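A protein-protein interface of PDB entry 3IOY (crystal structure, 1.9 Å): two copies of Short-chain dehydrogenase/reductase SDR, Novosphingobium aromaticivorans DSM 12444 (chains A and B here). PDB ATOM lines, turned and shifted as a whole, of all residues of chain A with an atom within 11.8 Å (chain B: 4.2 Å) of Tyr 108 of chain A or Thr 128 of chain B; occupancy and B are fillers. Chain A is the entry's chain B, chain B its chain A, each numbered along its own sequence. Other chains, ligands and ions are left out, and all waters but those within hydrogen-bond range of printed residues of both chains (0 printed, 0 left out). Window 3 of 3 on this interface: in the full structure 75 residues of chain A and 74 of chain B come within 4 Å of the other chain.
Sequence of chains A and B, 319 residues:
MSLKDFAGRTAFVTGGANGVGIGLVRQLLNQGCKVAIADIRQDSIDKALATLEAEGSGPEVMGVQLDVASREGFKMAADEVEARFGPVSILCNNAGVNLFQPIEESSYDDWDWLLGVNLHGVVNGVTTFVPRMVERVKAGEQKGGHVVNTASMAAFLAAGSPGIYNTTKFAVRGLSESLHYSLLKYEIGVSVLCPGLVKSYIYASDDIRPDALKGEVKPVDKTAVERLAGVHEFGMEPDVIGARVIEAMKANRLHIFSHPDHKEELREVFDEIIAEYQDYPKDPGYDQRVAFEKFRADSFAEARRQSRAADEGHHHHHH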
ATOM      1  N   VAL A  97     -23.063 -39.613 -29.722  1.00  0.00           N
ATOM      2  CA  VAL A  97     -22.068 -38.561 -29.900  1.00  0.00           C
ATOM      3  C   VAL A  97     -21.450 -38.213 -28.548  1.00  0.00           C
ATOM      4  O   VAL A  97     -22.083 -38.393 -27.492  1.00  0.00           O
ATOM      5  CB  VAL A  97     -22.669 -37.277 -30.571  1.00  0.00           C
ATOM      6  CG1 VAL A  97     -23.129 -37.568 -31.998  1.00  0.00           C
ATOM      7  CG2 VAL A  97     -23.809 -36.695 -29.726  1.00  0.00           C
ATOM      8  N   LEU A  99     -18.908 -35.156 -26.239  1.00  0.00           N
ATOM      9  CA  LEU A  99     -18.464 -33.748 -26.124  1.00  0.00           C
ATOM     10  C   LEU A  99     -17.662 -33.620 -24.838  1.00  0.00           C
ATOM     11  O   LEU A  99     -18.211 -33.767 -23.712  1.00  0.00           O
ATOM     12  CB  LEU A  99     -19.683 -32.809 -26.103  1.00  0.00           C
ATOM     13  CG  LEU A  99     -19.546 -31.289 -26.196  1.00  0.00           C
ATOM     14  CD1 LEU A  99     -18.656 -30.872 -27.401  1.00  0.00           C
ATOM     15  CD2 LEU A  99     -20.926 -30.635 -26.315  1.00  0.00           C
ATOM     16  N   GLN A 101     -16.464 -31.834 -22.158  1.00  0.00           N
ATOM     17  CA  GLN A 101     -16.723 -30.584 -21.456  1.00  0.00           C
ATOM     18  C   GLN A 101     -17.428 -30.940 -20.150  1.00  0.00           C
ATOM     19  O   GLN A 101     -18.266 -31.887 -20.137  1.00  0.00           O
ATOM     20  CB  GLN A 101     -17.692 -29.724 -22.260  1.00  0.00           C
ATOM     21  CG  GLN A 101     -17.146 -29.158 -23.572  1.00  0.00           C
ATOM     22  CD  GLN A 101     -18.195 -28.389 -24.351  1.00  0.00           C
ATOM     23  OE1 GLN A 101     -17.952 -27.984 -25.493  1.00  0.00           O
ATOM     24  NE2 GLN A 101     -19.375 -28.160 -23.732  1.00  0.00           N
ATOM     25  N   PRO A 102     -17.135 -30.178 -19.062  1.00  0.00           N
ATOM     26  CA  PRO A 102     -17.942 -30.277 -17.842  1.00  0.00           C
ATOM     27  C   PRO A 102     -19.288 -29.600 -18.035  1.00  0.00           C
ATOM     28  O   PRO A 102     -19.457 -28.762 -18.925  1.00  0.00           O
ATOM     29  CB  PRO A 102     -17.117 -29.507 -16.801  1.00  0.00           C
ATOM     30  CG  PRO A 102     -16.321 -28.516 -17.618  1.00  0.00           C
ATOM     31  CD  PRO A 102     -16.037 -29.187 -18.925  1.00  0.00           C
ATOM     32  N   ILE A 103     -20.249 -29.958 -17.211  1.00  0.00           N
ATOM     33  CA  ILE A 103     -21.576 -29.401 -17.352  1.00  0.00           C
ATOM     34  C   ILE A 103     -21.571 -27.847 -17.225  1.00  0.00           C
ATOM     35  O   ILE A 103     -22.201 -27.174 -18.036  1.00  0.00           O
ATOM     36  CB  ILE A 103     -22.562 -30.068 -16.362  1.00  0.00           C
ATOM     37  CG1 ILE A 103     -22.838 -31.525 -16.805  1.00  0.00           C
ATOM     38  CG2 ILE A 103     -23.826 -29.247 -16.232  1.00  0.00           C
ATOM     39  CD1 ILE A 103     -23.466 -32.425 -15.692  1.00  0.00           C
ATOM     40  N   GLU A 104     -20.873 -27.281 -16.237  1.00  0.00           N
ATOM     41  CA  GLU A 104     -20.990 -25.802 -16.029  1.00  0.00           C
ATOM     42  C   GLU A 104     -20.476 -24.980 -17.229  1.00  0.00           C
ATOM     43  O   GLU A 104     -20.833 -23.809 -17.383  1.00  0.00           O
ATOM     44  CB  GLU A 104     -20.347 -25.345 -14.714  1.00  0.00           C
ATOM     45  CG  GLU A 104     -18.794 -25.281 -14.692  1.00  0.00           C
ATOM     46  CD  GLU A 104     -18.147 -26.651 -14.526  1.00  0.00           C
ATOM     47  OE1 GLU A 104     -18.884 -27.652 -14.310  1.00  0.00           O
ATOM     48  OE2 GLU A 104     -16.907 -26.739 -14.619  1.00  0.00           O
ATOM     49  N   GLU A 105     -19.665 -25.611 -18.077  1.00  0.00           N
ATOM     50  CA  GLU A 105     -19.220 -25.012 -19.346  1.00  0.00           C
ATOM     51  C   GLU A 105     -20.070 -25.384 -20.582  1.00  0.00           C
ATOM     52  O   GLU A 105     -19.701 -25.077 -21.723  1.00  0.00           O
ATOM     53  CB  GLU A 105     -17.745 -25.347 -19.579  1.00  0.00           C
ATOM     54  CG  GLU A 105     -16.860 -24.771 -18.496  1.00  0.00           C
ATOM     55  CD  GLU A 105     -15.415 -25.230 -18.584  1.00  0.00           C
ATOM     56  OE1 GLU A 105     -15.000 -25.735 -19.661  1.00  0.00           O
ATOM     57  OE2 GLU A 105     -14.695 -25.087 -17.555  1.00  0.00           O
ATOM     58  N   SER A 106     -21.215 -26.037 -20.373  1.00  0.00           N
ATOM     59  CA  SER A 106     -21.999 -26.498 -21.530  1.00  0.00           C
ATOM     60  C   SER A 106     -23.260 -25.680 -21.699  1.00  0.00           C
ATOM     61  O   SER A 106     -23.932 -25.352 -20.729  1.00  0.00           O
ATOM     62  CB  SER A 106     -22.365 -27.990 -21.392  1.00  0.00           C
ATOM     63  OG  SER A 106     -21.194 -28.783 -21.233  1.00  0.00           O
ATOM     64  N   SER A 107     -23.608 -25.394 -22.940  1.00  0.00           N
ATOM     65  CA  SER A 107     -24.790 -24.583 -23.219  1.00  0.00           C
ATOM     66  C   SER A 107     -26.011 -25.456 -23.412  1.00  0.00           C
ATOM     67  O   SER A 107     -25.902 -26.679 -23.540  1.00  0.00           O
ATOM     68  CB  SER A 107     -24.568 -23.794 -24.501  1.00  0.00           C
ATOM     69  OG  SER A 107     -24.462 -24.715 -25.572  1.00  0.00           O
ATOM     70  N   TYR A 108     -27.179 -24.819 -23.451  1.00  0.00           N
ATOM     71  CA  TYR A 108     -28.391 -25.525 -23.824  1.00  0.00           C
ATOM     72  C   TYR A 108     -28.267 -26.189 -25.212  1.00  0.00           C
ATOM     73  O   TYR A 108     -28.746 -27.316 -25.409  1.00  0.00           O
ATOM     74  CB  TYR A 108     -29.591 -24.599 -23.782  1.00  0.00           C
ATOM     75  CG  TYR A 108     -30.117 -24.254 -22.416  1.00  0.00           C
ATOM     76  CD1 TYR A 108     -30.529 -25.250 -21.534  1.00  0.00           C
ATOM     77  CD2 TYR A 108     -30.292 -22.915 -22.038  1.00  0.00           C
ATOM     78  CE1 TYR A 108     -31.044 -24.937 -20.305  1.00  0.00           C
ATOM     79  CE2 TYR A 108     -30.835 -22.581 -20.802  1.00  0.00           C
ATOM     80  CZ  TYR A 108     -31.209 -23.596 -19.941  1.00  0.00           C
ATOM     81  OH  TYR A 108     -31.736 -23.302 -18.734  1.00  0.00           O
ATOM     82  N   ASP A 109     -27.598 -25.534 -26.166  1.00  0.00           N
ATOM     83  CA  ASP A 109     -27.385 -26.173 -27.481  1.00  0.00           C
ATOM     84  C   ASP A 109     -26.631 -27.509 -27.364  1.00  0.00           C
ATOM     85  O   ASP A 109     -26.954 -28.471 -28.071  1.00  0.00           O
ATOM     86  CB  ASP A 109     -26.649 -25.250 -28.466  1.00  0.00           C
ATOM     87  CG  ASP A 109     -27.510 -24.110 -28.955  1.00  0.00           C
ATOM     88  OD1 ASP A 109     -28.752 -24.197 -28.809  1.00  0.00           O
ATOM     89  OD2 ASP A 109     -26.944 -23.134 -29.507  1.00  0.00           O
ATOM     90  N   ASP A 110     -25.634 -27.545 -26.480  1.00  0.00           N
ATOM     91  CA  ASP A 110     -24.850 -28.769 -26.189  1.00  0.00           C
ATOM     92  C   ASP A 110     -25.749 -29.881 -25.607  1.00  0.00           C
ATOM     93  O   ASP A 110     -25.648 -31.050 -26.028  1.00  0.00           O
ATOM     94  CB  ASP A 110     -23.732 -28.497 -25.177  1.00  0.00           C
ATOM     95  CG  ASP A 110     -22.684 -27.499 -25.683  1.00  0.00           C
ATOM     96  OD1 ASP A 110     -22.484 -27.426 -26.909  1.00  0.00           O
ATOM     97  OD2 ASP A 110     -22.051 -26.822 -24.827  1.00  0.00           O
ATOM     98  N   TRP A 111     -26.591 -29.514 -24.643  1.00  0.00           N
ATOM     99  CA  TRP A 111     -27.573 -30.445 -24.076  1.00  0.00           C
ATOM    100  C   TRP A 111     -28.501 -30.981 -25.169  1.00  0.00           C
ATOM    101  O   TRP A 111     -28.705 -32.198 -25.279  1.00  0.00           O
ATOM    102  CB  TRP A 111     -28.405 -29.795 -22.951  1.00  0.00           C
ATOM    103  CG  TRP A 111     -27.723 -29.744 -21.573  1.00  0.00           C
ATOM    104  CD1 TRP A 111     -27.174 -28.647 -20.954  1.00  0.00           C
ATOM    105  CD2 TRP A 111     -27.537 -30.845 -20.675  1.00  0.00           C
ATOM    106  NE1 TRP A 111     -26.652 -29.009 -19.731  1.00  0.00           N
ATOM    107  CE2 TRP A 111     -26.876 -30.349 -19.532  1.00  0.00           C
ATOM    108  CE3 TRP A 111     -27.907 -32.215 -20.717  1.00  0.00           C
ATOM    109  CZ2 TRP A 111     -26.541 -31.172 -18.433  1.00  0.00           C
ATOM    110  CZ3 TRP A 111     -27.557 -33.048 -19.620  1.00  0.00           C
ATOM    111  CH2 TRP A 111     -26.868 -32.526 -18.515  1.00  0.00           C
ATOM    112  N   ASP A 112     -29.037 -30.083 -26.003  1.00  0.00           N
ATOM    113  CA  ASP A 112     -30.009 -30.504 -27.018  1.00  0.00           C
ATOM    114  C   ASP A 112     -29.404 -31.461 -28.020  1.00  0.00           C
ATOM    115  O   ASP A 112     -30.027 -32.452 -28.368  1.00  0.00           O
ATOM    116  CB  ASP A 112     -30.660 -29.305 -27.705  1.00  0.00           C
ATOM    117  CG  ASP A 112     -31.536 -28.526 -26.771  1.00  0.00           C
ATOM    118  OD1 ASP A 112     -31.902 -29.044 -25.690  1.00  0.00           O
ATOM    119  OD2 ASP A 112     -31.870 -27.368 -27.087  1.00  0.00           O
ATOM    120  N   TRP A 113     -28.182 -31.178 -28.458  1.00  0.00           N
ATOM    121  CA  TRP A 113     -27.465 -32.074 -29.361  1.00  0.00           C
ATOM    122  C   TRP A 113     -27.226 -33.492 -28.809  1.00  0.00           C
ATOM    123  O   TRP A 113     -27.540 -34.501 -29.459  1.00  0.00           O
ATOM    124  CB  TRP A 113     -26.126 -31.434 -29.770  1.00  0.00           C
ATOM    125  CG  TRP A 113     -25.343 -32.279 -30.714  1.00  0.00           C
ATOM    126  CD1 TRP A 113     -25.827 -33.021 -31.769  1.00  0.00           C
ATOM    127  CD2 TRP A 113     -23.936 -32.466 -30.712  1.00  0.00           C
ATOM    128  NE1 TRP A 113     -24.800 -33.659 -32.409  1.00  0.00           N
ATOM    129  CE2 TRP A 113     -23.625 -33.334 -31.787  1.00  0.00           C
ATOM    130  CE3 TRP A 113     -22.896 -31.972 -29.917  1.00  0.00           C
ATOM    131  CZ2 TRP A 113     -22.317 -33.735 -32.075  1.00  0.00           C
ATOM    132  CZ3 TRP A 113     -21.594 -32.377 -30.199  1.00  0.00           C
ATOM    133  CH2 TRP A 113     -21.319 -33.253 -31.273  1.00  0.00           C
ATOM    134  N   LEU A 114     -26.645 -33.572 -27.619  1.00  0.00           N
ATOM    135  CA  LEU A 114     -26.286 -34.871 -27.049  1.00  0.00           C
ATOM    136  C   LEU A 114     -27.494 -35.641 -26.541  1.00  0.00           C
ATOM    137  O   LEU A 114     -27.560 -36.856 -26.721  1.00  0.00           O
ATOM    138  CB  LEU A 114     -25.221 -34.719 -25.950  1.00  0.00           C
ATOM    139  CG  LEU A 114     -23.820 -35.132 -26.366  1.00  0.00           C
ATOM    140  CD1 LEU A 114     -23.289 -34.098 -27.336  1.00  0.00           C
ATOM    141  CD2 LEU A 114     -22.872 -35.254 -25.178  1.00  0.00           C
ATOM    142  N   LEU A 115     -28.454 -34.954 -25.926  1.00  0.00           N
ATOM    143  CA  LEU A 115     -29.712 -35.605 -25.542  1.00  0.00           C
ATOM    144  C   LEU A 115     -30.413 -36.158 -26.790  1.00  0.00           C
ATOM    145  O   LEU A 115     -30.947 -37.277 -26.782  1.00  0.00           O
ATOM    146  CB  LEU A 115     -30.639 -34.622 -24.826  1.00  0.00           C
ATOM    147  CG  LEU A 115     -30.284 -34.241 -23.387  1.00  0.00           C
ATOM    148  CD1 LEU A 115     -31.219 -33.107 -22.855  1.00  0.00           C
ATOM    149  CD2 LEU A 115     -30.313 -35.491 -22.482  1.00  0.00           C
ATOM    150  N   GLY A 116     -30.371 -35.368 -27.878  1.00  0.00           N
ATOM    151  CA  GLY A 116     -31.008 -35.745 -29.122  1.00  0.00           C
ATOM    152  C   GLY A 116     -30.522 -37.088 -29.618  1.00  0.00           C
ATOM    153  O   GLY A 116     -31.318 -37.987 -29.857  1.00  0.00           O
ATOM    154  N   VAL A 117     -29.218 -37.206 -29.815  1.00  0.00           N
ATOM    155  CA  VAL A 117     -28.638 -38.461 -30.277  1.00  0.00           C
ATOM    156  C   VAL A 117     -28.671 -39.585 -29.236  1.00  0.00           C
ATOM    157  O   VAL A 117     -29.135 -40.689 -29.538  1.00  0.00           O
ATOM    158  CB  VAL A 117     -27.209 -38.252 -30.812  1.00  0.00           C
ATOM    159  CG1 VAL A 117     -26.584 -39.564 -31.304  1.00  0.00           C
ATOM    160  CG2 VAL A 117     -27.244 -37.234 -31.982  1.00  0.00           C
ATOM    161  N   HIS A 120     -32.665 -39.480 -26.886  1.00  0.00           N
ATOM    162  CA  HIS A 120     -33.858 -39.495 -27.754  1.00  0.00           C
ATOM    163  C   HIS A 120     -33.739 -40.542 -28.813  1.00  0.00           C
ATOM    164  O   HIS A 120     -34.737 -41.168 -29.136  1.00  0.00           O
ATOM    165  CB  HIS A 120     -34.161 -38.109 -28.335  1.00  0.00           C
ATOM    166  CG  HIS A 120     -34.597 -37.132 -27.294  1.00  0.00           C
ATOM    167  ND1 HIS A 120     -35.795 -37.259 -26.616  1.00  0.00           N
ATOM    168  CD2 HIS A 120     -33.983 -36.044 -26.774  1.00  0.00           C
ATOM    169  CE1 HIS A 120     -35.906 -36.275 -25.739  1.00  0.00           C
ATOM    170  NE2 HIS A 120     -34.815 -35.532 -25.804  1.00  0.00           N
ATOM    171  N   ILE A 164     -22.444 -34.041 -19.739  1.00  0.00           N
ATOM    172  CA  ILE A 164     -23.667 -34.285 -20.500  1.00  0.00           C
ATOM    173  C   ILE A 164     -23.638 -35.720 -21.038  1.00  0.00           C
ATOM    174  O   ILE A 164     -24.633 -36.428 -20.918  1.00  0.00           O
ATOM    175  CB  ILE A 164     -23.877 -33.293 -21.694  1.00  0.00           C
ATOM    176  CG1 ILE A 164     -24.000 -31.856 -21.199  1.00  0.00           C
ATOM    177  CG2 ILE A 164     -25.136 -33.689 -22.520  1.00  0.00           C
ATOM    178  CD1 ILE A 164     -24.159 -30.813 -22.341  1.00  0.00           C
ATOM    179  N   TYR A 165     -22.507 -36.138 -21.637  1.00  0.00           N
ATOM    180  CA  TYR A 165     -22.369 -37.513 -22.100  1.00  0.00           C
ATOM    181  C   TYR A 165     -22.697 -38.513 -21.002  1.00  0.00           C
ATOM    182  O   TYR A 165     -23.473 -39.478 -21.253  1.00  0.00           O
ATOM    183  CB  TYR A 165     -20.973 -37.784 -22.630  1.00  0.00           C
ATOM    184  CG  TYR A 165     -20.759 -39.166 -23.211  1.00  0.00           C
ATOM    185  CD1 TYR A 165     -21.129 -39.448 -24.525  1.00  0.00           C
ATOM    186  CD2 TYR A 165     -20.152 -40.189 -22.452  1.00  0.00           C
ATOM    187  CE1 TYR A 165     -20.880 -40.714 -25.091  1.00  0.00           C
ATOM    188  CE2 TYR A 165     -19.904 -41.456 -23.018  1.00  0.00           C
ATOM    189  CZ  TYR A 165     -20.286 -41.697 -24.317  1.00  0.00           C
ATOM    190  OH  TYR A 165     -20.089 -42.919 -24.876  1.00  0.00           O
ATOM    191  N   THR A 168     -26.402 -38.672 -20.304  1.00  0.00           N
ATOM    192  CA  THR A 168     -27.153 -39.451 -21.306  1.00  0.00           C
ATOM    193  C   THR A 168     -26.933 -40.965 -21.135  1.00  0.00           C
ATOM    194  O   THR A 168     -27.854 -41.774 -21.372  1.00  0.00           O
ATOM    195  CB  THR A 168     -26.816 -39.056 -22.772  1.00  0.00           C
ATOM    196  OG1 THR A 168     -25.497 -39.480 -23.090  1.00  0.00           O
ATOM    197  CG2 THR A 168     -26.935 -37.529 -23.032  1.00  0.00           C
ATOM    198  N   ARG B  71     -37.045 -23.130 -20.015  1.00  0.00           N
ATOM    199  CA  ARG B  71     -35.768 -22.449 -19.799  1.00  0.00           C
ATOM    200  C   ARG B  71     -35.978 -20.947 -19.572  1.00  0.00           C
ATOM    201  O   ARG B  71     -35.431 -20.344 -18.648  1.00  0.00           O
ATOM    202  CB  ARG B  71     -34.858 -22.665 -20.998  1.00  0.00           C
ATOM    203  CG  ARG B  71     -34.480 -24.114 -21.103  1.00  0.00           C
ATOM    204  CD  ARG B  71     -33.965 -24.457 -22.459  1.00  0.00           C
ATOM    205  NE  ARG B  71     -33.464 -25.825 -22.454  1.00  0.00           N
ATOM    206  CZ  ARG B  71     -32.892 -26.411 -23.503  1.00  0.00           C
ATOM    207  NH1 ARG B  71     -32.782 -25.754 -24.645  1.00  0.00           N
ATOM    208  NH2 ARG B  71     -32.451 -27.660 -23.416  1.00  0.00           N
ATOM    209  N   PHE B  74     -37.474 -20.344 -16.129  1.00  0.00           N
ATOM    210  CA  PHE B  74     -36.448 -20.522 -15.081  1.00  0.00           C
ATOM    211  C   PHE B  74     -35.536 -19.270 -14.983  1.00  0.00           C
ATOM    212  O   PHE B  74     -35.234 -18.817 -13.876  1.00  0.00           O
ATOM    213  CB  PHE B  74     -35.620 -21.798 -15.340  1.00  0.00           C
ATOM    214  CG  PHE B  74     -35.364 -22.633 -14.098  1.00  0.00           C
ATOM    215  CD1 PHE B  74     -35.787 -23.974 -14.045  1.00  0.00           C
ATOM    216  CD2 PHE B  74     -34.706 -22.093 -12.993  1.00  0.00           C
ATOM    217  CE1 PHE B  74     -35.561 -24.760 -12.928  1.00  0.00           C
ATOM    218  CE2 PHE B  74     -34.485 -22.882 -11.835  1.00  0.00           C
ATOM    219  CZ  PHE B  74     -34.906 -24.218 -11.816  1.00  0.00           C
ATOM    220  N   LYS B  75     -35.093 -18.732 -16.117  1.00  0.00           N
ATOM    221  CA  LYS B  75     -34.290 -17.488 -16.106  1.00  0.00           C
ATOM    222  C   LYS B  75     -35.052 -16.314 -15.444  1.00  0.00           C
ATOM    223  O   LYS B  75     -34.537 -15.618 -14.530  1.00  0.00           O
ATOM    224  CB  LYS B  75     -33.894 -17.115 -17.522  1.00  0.00           C
ATOM    225  CG  LYS B  75     -32.541 -16.467 -17.589  1.00  0.00           C
ATOM    226  CD  LYS B  75     -32.575 -15.170 -18.330  1.00  0.00           C
ATOM    227  CE  LYS B  75     -31.243 -14.452 -18.124  1.00  0.00           C
ATOM    228  NZ  LYS B  75     -31.467 -13.049 -17.735  1.00  0.00           N
ATOM    229  N   ALA B  78     -35.353 -16.841 -11.669  1.00  0.00           N
ATOM    230  CA  ALA B  78     -34.028 -16.618 -11.046  1.00  0.00           C
ATOM    231  C   ALA B  78     -33.719 -15.113 -10.894  1.00  0.00           C
ATOM    232  O   ALA B  78     -33.301 -14.663  -9.806  1.00  0.00           O
ATOM    233  CB  ALA B  78     -32.957 -17.257 -11.871  1.00  0.00           C
ATOM    234  N   ASN B 124     -32.141 -27.260 -16.448  1.00  0.00           N
ATOM    235  CA  ASN B 124     -32.498 -25.844 -16.537  1.00  0.00           C
ATOM    236  C   ASN B 124     -32.063 -25.118 -15.253  1.00  0.00           C
ATOM    237  O   ASN B 124     -31.520 -24.006 -15.297  1.00  0.00           O
ATOM    238  CB  ASN B 124     -34.021 -25.734 -16.716  1.00  0.00           C
ATOM    239  CG  ASN B 124     -34.491 -26.132 -18.104  1.00  0.00           C
ATOM    240  OD1 ASN B 124     -33.683 -26.394 -19.015  1.00  0.00           O
ATOM    241  ND2 ASN B 124     -35.829 -26.202 -18.271  1.00  0.00           N
ATOM    242  N   GLY B 125     -32.316 -25.740 -14.103  1.00  0.00           N
ATOM    243  CA  GLY B 125     -31.862 -25.202 -12.800  1.00  0.00           C
ATOM    244  C   GLY B 125     -30.346 -25.028 -12.810  1.00  0.00           C
ATOM    245  O   GLY B 125     -29.795 -23.939 -12.531  1.00  0.00           O
ATOM    246  N   VAL B 126     -29.666 -26.114 -13.126  1.00  0.00           N
ATOM    247  CA  VAL B 126     -28.225 -26.075 -13.178  1.00  0.00           C
ATOM    248  C   VAL B 126     -27.716 -25.026 -14.183  1.00  0.00           C
ATOM    249  O   VAL B 126     -26.837 -24.220 -13.848  1.00  0.00           O
ATOM    250  CB  VAL B 126     -27.656 -27.477 -13.433  1.00  0.00           C
ATOM    251  CG1 VAL B 126     -26.191 -27.393 -13.828  1.00  0.00           C
ATOM    252  CG2 VAL B 126     -27.837 -28.300 -12.191  1.00  0.00           C
ATOM    253  N   THR B 127     -28.287 -24.994 -15.381  1.00  0.00           N
ATOM    254  CA  THR B 127     -27.805 -24.098 -16.440  1.00  0.00           C
ATOM    255  C   THR B 127     -28.129 -22.627 -16.119  1.00  0.00           C
ATOM    256  O   THR B 127     -27.340 -21.741 -16.435  1.00  0.00           O
ATOM    257  CB  THR B 127     -28.326 -24.488 -17.852  1.00  0.00           C
ATOM    258  OG1 THR B 127     -27.989 -25.859 -18.114  1.00  0.00           O
ATOM    259  CG2 THR B 127     -27.694 -23.642 -18.945  1.00  0.00           C
ATOM    260  N   THR B 128     -29.231 -22.387 -15.418  1.00  0.00           N
ATOM    261  CA  THR B 128     -29.621 -21.017 -15.034  1.00  0.00           C
ATOM    262  C   THR B 128     -28.712 -20.453 -13.930  1.00  0.00           C
ATOM    263  O   THR B 128     -28.365 -19.268 -13.941  1.00  0.00           O
ATOM    264  CB  THR B 128     -31.100 -21.009 -14.532  1.00  0.00           C
ATOM    265  OG1 THR B 128     -31.937 -21.485 -15.591  1.00  0.00           O
ATOM    266  CG2 THR B 128     -31.578 -19.589 -14.147  1.00  0.00           C
ATOM    267  N   PHE B 129     -28.371 -21.290 -12.957  1.00  0.00           N
ATOM    268  CA  PHE B 129     -27.792 -20.799 -11.707  1.00  0.00           C
ATOM    269  C   PHE B 129     -26.308 -21.054 -11.554  1.00  0.00           C
ATOM    270  O   PHE B 129     -25.589 -20.208 -11.012  1.00  0.00           O
ATOM    271  CB  PHE B 129     -28.499 -21.389 -10.506  1.00  0.00           C
ATOM    272  CG  PHE B 129     -29.691 -20.615 -10.057  1.00  0.00           C
ATOM    273  CD1 PHE B 129     -30.951 -21.196 -10.089  1.00  0.00           C
ATOM    274  CD2 PHE B 129     -29.557 -19.299  -9.562  1.00  0.00           C
ATOM    275  CE1 PHE B 129     -32.067 -20.497  -9.667  1.00  0.00           C
ATOM    276  CE2 PHE B 129     -30.674 -18.585  -9.135  1.00  0.00           C
ATOM    277  CZ  PHE B 129     -31.934 -19.183  -9.171  1.00  0.00           C
ATOM    278  N   VAL B 130     -25.849 -22.230 -11.975  1.00  0.00           N
ATOM    279  CA  VAL B 130     -24.453 -22.645 -11.727  1.00  0.00           C
ATOM    280  C   VAL B 130     -23.427 -21.720 -12.398  1.00  0.00           C
ATOM    281  O   VAL B 130     -22.426 -21.388 -11.762  1.00  0.00           O
ATOM    282  CB  VAL B 130     -24.194 -24.150 -12.064  1.00  0.00           C
ATOM    283  CG1 VAL B 130     -22.681 -24.465 -12.186  1.00  0.00           C
ATOM    284  CG2 VAL B 130     -24.815 -25.054 -11.000  1.00  0.00           C
ATOM    285  N   ARG B 132     -23.785 -18.611 -13.106  1.00  0.00           N
ATOM    286  CA  ARG B 132     -23.804 -17.416 -12.274  1.00  0.00           C
ATOM    287  C   ARG B 132     -22.923 -17.631 -11.047  1.00  0.00           C
ATOM    288  O   ARG B 132     -22.079 -16.768 -10.730  1.00  0.00           O
ATOM    289  CB  ARG B 132     -25.215 -17.061 -11.793  1.00  0.00           C
ATOM    290  CG  ARG B 132     -26.266 -16.795 -12.869  1.00  0.00           C
ATOM    291  CD  ARG B 132     -27.620 -16.444 -12.220  1.00  0.00           C
ATOM    292  NE  ARG B 132     -28.659 -16.421 -13.253  1.00  0.00           N
ATOM    293  CZ  ARG B 132     -29.761 -15.673 -13.243  1.00  0.00           C
ATOM    294  NH1 ARG B 132     -30.018 -14.833 -12.234  1.00  0.00           N
ATOM    295  NH2 ARG B 132     -30.616 -15.760 -14.266  1.00  0.00           N
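Printed residues of chain B within 4 Å of Ile 103 of chain A: Val 126. Of the printed residues of chain B, Glu 104 of chain A touches Val 130 (3.6 Å). Asp 109 of chain A touches none of the printed residues of chain B. Of the printed residues of chain B, Trp 111 of chain A touches Thr 127. Printed residues of chain B within 4 Å of Asp 112 of chain A: Arg 71 (2.7 Å). Leu 115 of chain A touches none of the printed residues of chain B. Arg 71 of chain B touches just these residues of chain A: Tyr 108 (3.1 Å) and Asp 112 (2.7 Å). No residue of chain A comes within 4 Å of Phe 74 of chain B. No residue of chain A comes within 4 Å of Lys 75 of chain B. No residue of chain A comes within 4 Å of Ala 78 of chain B. No residue of chain A comes within 4 Å of Gly 125 of chain B. Val 126 of chain B touches just one residue of chain A: Ile 103. Thr 127 of chain B touches just these residues of chain A: Tyr 108 (3.7 Å) and Trp 111 (3.8 Å). Thr 128 of chain B touches just one residue of chain A: Tyr 108 (3.6 Å). Phe 129 of chain B touches none of the printed residues of chain A. Of chain A, only Glu 104 (3.6 Å) comes within 4 Å of Val 130 of chain B. No residue of chain A comes within 4 Å of Arg 132 of chain B. The nearest printed residue of chain B that does not touch Tyr 108 of chain A is Gly 125 of chain B (5.3 Å). The nearest residue of chain A that does not touch Thr 128 of chain B is Ser 106 of chain A (8.1 Å). The nearest printed residue of chain B that does not touch Asp 112 of chain A is Asn 124 of chain B (7.4 Å).
Printed residues of chain A that touch a printed residue of chain B: Ile 103, Glu 104, Tyr 108, Trp 111 and Asp 112. Hydrophobic or aromatic side chains of chain A that line the printed part of chain B: Ile 103, Tyr 108 and Trp 111. Of the 12 printed residues of chain B, 6 touch a printed residue of chain A. Printed residues of chain B that touch a printed residue of chain A: Arg 71, Asn 124, Val 126, Thr 127, Thr 128 and Val 130. Among the printed residues, 8 pairs touch across the chains.
OD1 of Asp 112 of chain A is in salt-bridge range of NH2 of Arg 71 of chain B, 2.7 Å away.
No position is printed for both chains.
Among the printed residues, pairs that only touch across the chains: Tyr 108 of chain A with Arg 71 of chain B, Tyr 108 of chain A with Asn 124 of chain B, Glu 104 of chain A with Val 130 of chain B, Tyr 108 of chain A with Thr 128 of chain B, Tyr 108 of chain A with Thr 127 of chain B, Trp 111 of chain A with Thr 127 of chain B and Ile 103 of chain A with Val 126 of chain B.
O of Asn 124 of chain B sits at hydrogen-bond distance from OG1 of Thr 128 of chain B. The guanidinium group of Arg 71 of chain B lies close to the side-chain amide oxygen of Asn 124 of chain B (3.5 Å). The backbone carbonyl oxygen of Thr 128 of chain B is in hydrogen-bond range of the guanidinium group of Arg 132 of chain B, at 2.9 Å.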
